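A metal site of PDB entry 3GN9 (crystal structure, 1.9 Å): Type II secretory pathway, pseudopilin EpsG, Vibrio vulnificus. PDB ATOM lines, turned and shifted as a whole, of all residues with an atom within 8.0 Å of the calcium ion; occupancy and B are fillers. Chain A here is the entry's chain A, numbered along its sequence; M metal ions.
Along chain A the residues within 4 Å of the calcium ion span positions 91 to 105.
The nearest printed residue that does not touch the calcium ion is Glu 97 (4.1 Å).
The calcium ion is bound by O of Ala 103 (2.2 Å).
The calcium ion is bound by O of Gln 96 (2.2 Å).
O of Leu 91 is bound to the calcium ion, at 2.3 Å.
O of Gly 98 binds the calcium ion (2.4 Å).
The calcium ion is bound by OD1 of Asp 105, 2.4 Å away.
The calcium ion is bound by OD1 of Asp 94 (2.6 Å).
The calcium ion has six donor atoms within binding distance.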
ATOM      1  N   THR A  90      32.405  -1.309 -18.685  1.00  0.00           N
ATOM      2  CA  THR A  90      31.849  -0.381 -19.664  1.00  0.00           C
ATOM      3  C   THR A  90      30.720   0.369 -19.005  1.00  0.00           C
ATOM      4  O   THR A  90      29.938  -0.231 -18.268  1.00  0.00           O
ATOM      5  CB  THR A  90      31.322  -1.099 -20.958  1.00  0.00           C
ATOM      6  OG1 THR A  90      30.633  -0.147 -21.771  1.00  0.00           O
ATOM      7  CG2 THR A  90      30.408  -2.308 -20.665  1.00  0.00           C
ATOM      8  N   LEU A  91      30.644   1.679 -19.236  1.00  0.00           N
ATOM      9  CA  LEU A  91      29.500   2.459 -18.716  1.00  0.00           C
ATOM     10  C   LEU A  91      28.227   2.320 -19.561  1.00  0.00           C
ATOM     11  O   LEU A  91      27.261   3.071 -19.344  1.00  0.00           O
ATOM     12  CB  LEU A  91      29.893   3.948 -18.569  1.00  0.00           C
ATOM     13  CG  LEU A  91      30.976   4.258 -17.531  1.00  0.00           C
ATOM     14  CD1 LEU A  91      31.266   5.750 -17.484  1.00  0.00           C
ATOM     15  CD2 LEU A  91      30.570   3.750 -16.160  1.00  0.00           C
ATOM     16  N   GLY A  92      28.205   1.392 -20.501  1.00  0.00           N
ATOM     17  CA  GLY A  92      26.999   1.115 -21.272  1.00  0.00           C
ATOM     18  C   GLY A  92      26.728   2.159 -22.352  1.00  0.00           C
ATOM     19  O   GLY A  92      27.568   3.021 -22.644  1.00  0.00           O
ATOM     20  N   ALA A  93      25.532   2.073 -22.924  1.00  0.00           N
ATOM     21  CA  ALA A  93      25.162   2.864 -24.098  1.00  0.00           C
ATOM     22  C   ALA A  93      25.264   4.380 -23.886  1.00  0.00           C
ATOM     23  O   ALA A  93      25.501   5.130 -24.829  1.00  0.00           O
ATOM     24  CB  ALA A  93      23.757   2.491 -24.556  1.00  0.00           C
ATOM     25  N   ASP A  94      25.084   4.819 -22.640  1.00  0.00           N
ATOM     26  CA  ASP A  94      25.001   6.246 -22.356  1.00  0.00           C
ATOM     27  C   ASP A  94      26.362   6.859 -22.061  1.00  0.00           C
ATOM     28  O   ASP A  94      26.478   8.074 -21.923  1.00  0.00           O
ATOM     29  CB  ASP A  94      24.014   6.531 -21.202  1.00  0.00           C
ATOM     30  CG  ASP A  94      24.429   5.883 -19.886  1.00  0.00           C
ATOM     31  OD1 ASP A  94      25.425   5.135 -19.863  1.00  0.00           O
ATOM     32  OD2 ASP A  94      23.741   6.125 -18.873  1.00  0.00           O
ATOM     33  N   GLY A  95      27.378   6.009 -21.958  1.00  0.00           N
ATOM     34  CA  GLY A  95      28.731   6.472 -21.699  1.00  0.00           C
ATOM     35  C   GLY A  95      28.871   7.146 -20.349  1.00  0.00           C
ATOM     36  O   GLY A  95      29.755   7.971 -20.154  1.00  0.00           O
ATOM     37  N   GLN A  96      28.005   6.777 -19.408  1.00  0.00           N
ATOM     38  CA  GLN A  96      27.930   7.437 -18.116  1.00  0.00           C
ATOM     39  C   GLN A  96      27.501   6.451 -17.023  1.00  0.00           C
ATOM     40  O   GLN A  96      26.951   5.380 -17.322  1.00  0.00           O
ATOM     41  CB  GLN A  96      26.950   8.614 -18.203  1.00  0.00           C
ATOM     42  CG  GLN A  96      27.160   9.679 -17.129  1.00  0.00           C
ATOM     43  CD  GLN A  96      26.512  11.009 -17.455  1.00  0.00           C
ATOM     44  OE1 GLN A  96      25.380  11.069 -17.969  1.00  0.00           O
ATOM     45  NE2 GLN A  96      27.218  12.089 -17.149  1.00  0.00           N
ATOM     46  N   GLU A  97      27.755   6.806 -15.769  1.00  0.00           N
ATOM     47  CA  GLU A  97      27.497   5.927 -14.628  1.00  0.00           C
ATOM     48  C   GLU A  97      26.018   5.782 -14.358  1.00  0.00           C
ATOM     49  O   GLU A  97      25.261   6.749 -14.437  1.00  0.00           O
ATOM     50  CB  GLU A  97      28.203   6.443 -13.376  1.00  0.00           C
ATOM     51  CG  GLU A  97      28.080   5.503 -12.185  1.00  0.00           C
ATOM     52  CD  GLU A  97      28.969   5.890 -11.022  1.00  0.00           C
ATOM     53  OE1 GLU A  97      30.215   5.862 -11.174  1.00  0.00           O
ATOM     54  OE2 GLU A  97      28.409   6.194  -9.945  1.00  0.00           O
ATOM     55  N   GLY A  98      25.601   4.564 -14.015  1.00  0.00           N
ATOM     56  CA  GLY A  98      24.192   4.262 -13.798  1.00  0.00           C
ATOM     57  C   GLY A  98      23.434   4.085 -15.097  1.00  0.00           C
ATOM     58  O   GLY A  98      23.979   4.269 -16.188  1.00  0.00           O
ATOM     59  N   GLY A  99      22.165   3.730 -14.978  1.00  0.00           N
ATOM     60  CA  GLY A  99      21.309   3.498 -16.137  1.00  0.00           C
ATOM     61  C   GLY A  99      20.800   2.061 -16.161  1.00  0.00           C
ATOM     62  O   GLY A  99      21.362   1.175 -15.513  1.00  0.00           O
ATOM     63  N   GLU A 100      19.744   1.861 -16.943  1.00  0.00           N
ATOM     64  CA  GLU A 100      19.098   0.568 -17.080  1.00  0.00           C
ATOM     65  C   GLU A 100      19.039   0.233 -18.565  1.00  0.00           C
ATOM     66  O   GLU A 100      19.336   1.085 -19.412  1.00  0.00           O
ATOM     67  CB  GLU A 100      17.670   0.632 -16.505  1.00  0.00           C
ATOM     68  CG  GLU A 100      17.218  -0.628 -15.794  1.00  0.00           C
ATOM     69  CD  GLU A 100      15.836  -0.469 -15.196  1.00  0.00           C
ATOM     70  OE1 GLU A 100      14.891  -0.204 -15.952  1.00  0.00           O
ATOM     71  OE2 GLU A 100      15.716  -0.594 -13.955  1.00  0.00           O
ATOM     72  N   GLY A 101      18.662  -0.993 -18.889  1.00  0.00           N
ATOM     73  CA  GLY A 101      18.625  -1.418 -20.287  1.00  0.00           C
ATOM     74  C   GLY A 101      20.017  -1.341 -20.860  1.00  0.00           C
ATOM     75  O   GLY A 101      20.974  -1.727 -20.197  1.00  0.00           O
ATOM     76  N   ALA A 102      20.135  -0.818 -22.087  1.00  0.00           N
ATOM     77  CA  ALA A 102      21.434  -0.762 -22.779  1.00  0.00           C
ATOM     78  C   ALA A 102      22.440   0.227 -22.139  1.00  0.00           C
ATOM     79  O   ALA A 102      23.641   0.156 -22.409  1.00  0.00           O
ATOM     80  CB  ALA A 102      21.234  -0.432 -24.262  1.00  0.00           C
ATOM     81  N   ALA A 103      21.940   1.139 -21.315  1.00  0.00           N
ATOM     82  CA  ALA A 103      22.791   2.112 -20.624  1.00  0.00           C
ATOM     83  C   ALA A 103      23.405   1.576 -19.322  1.00  0.00           C
ATOM     84  O   ALA A 103      24.209   2.254 -18.687  1.00  0.00           O
ATOM     85  CB  ALA A 103      22.016   3.387 -20.344  1.00  0.00           C
ATOM     86  N   ALA A 104      23.031   0.350 -18.916  1.00  0.00           N
ATOM     87  CA  ALA A 104      23.467  -0.186 -17.632  1.00  0.00           C
ATOM     88  C   ALA A 104      24.967  -0.392 -17.695  1.00  0.00           C
ATOM     89  O   ALA A 104      25.474  -0.655 -18.761  1.00  0.00           O
ATOM     90  CB  ALA A 104      22.787  -1.499 -17.336  1.00  0.00           C
ATOM     91  N   ASP A 105      25.649  -0.249 -16.570  1.00  0.00           N
ATOM     92  CA  ASP A 105      27.094  -0.483 -16.511  1.00  0.00           C
ATOM     93  C   ASP A 105      27.335  -1.963 -16.348  1.00  0.00           C
ATOM     94  O   ASP A 105      26.651  -2.626 -15.594  1.00  0.00           O
ATOM     95  CB  ASP A 105      27.680   0.287 -15.339  1.00  0.00           C
ATOM     96  CG  ASP A 105      27.333   1.755 -15.409  1.00  0.00           C
ATOM     97  OD1 ASP A 105      27.189   2.257 -16.550  1.00  0.00           O
ATOM     98  OD2 ASP A 105      27.174   2.394 -14.343  1.00  0.00           O
ATOM     99  N   ILE A 106      28.334  -2.482 -17.044  1.00  0.00           N
ATOM    100  CA  ILE A 106      28.631  -3.896 -16.956  1.00  0.00           C
ATOM    101  C   ILE A 106      30.098  -3.919 -16.590  1.00  0.00           C
ATOM    102  O   ILE A 106      30.907  -3.307 -17.295  1.00  0.00           O
ATOM    103  CB  ILE A 106      28.396  -4.629 -18.308  1.00  0.00           C
ATOM    104  CG1 ILE A 106      26.948  -4.468 -18.800  1.00  0.00           C
ATOM    105  CG2 ILE A 106      28.707  -6.121 -18.185  1.00  0.00           C
ATOM    106  CD1 ILE A 106      26.764  -4.983 -20.222  1.00  0.00           C
HETATM  107 CA    CA M   1      25.648   3.636 -17.799  1.00  0.00          CA
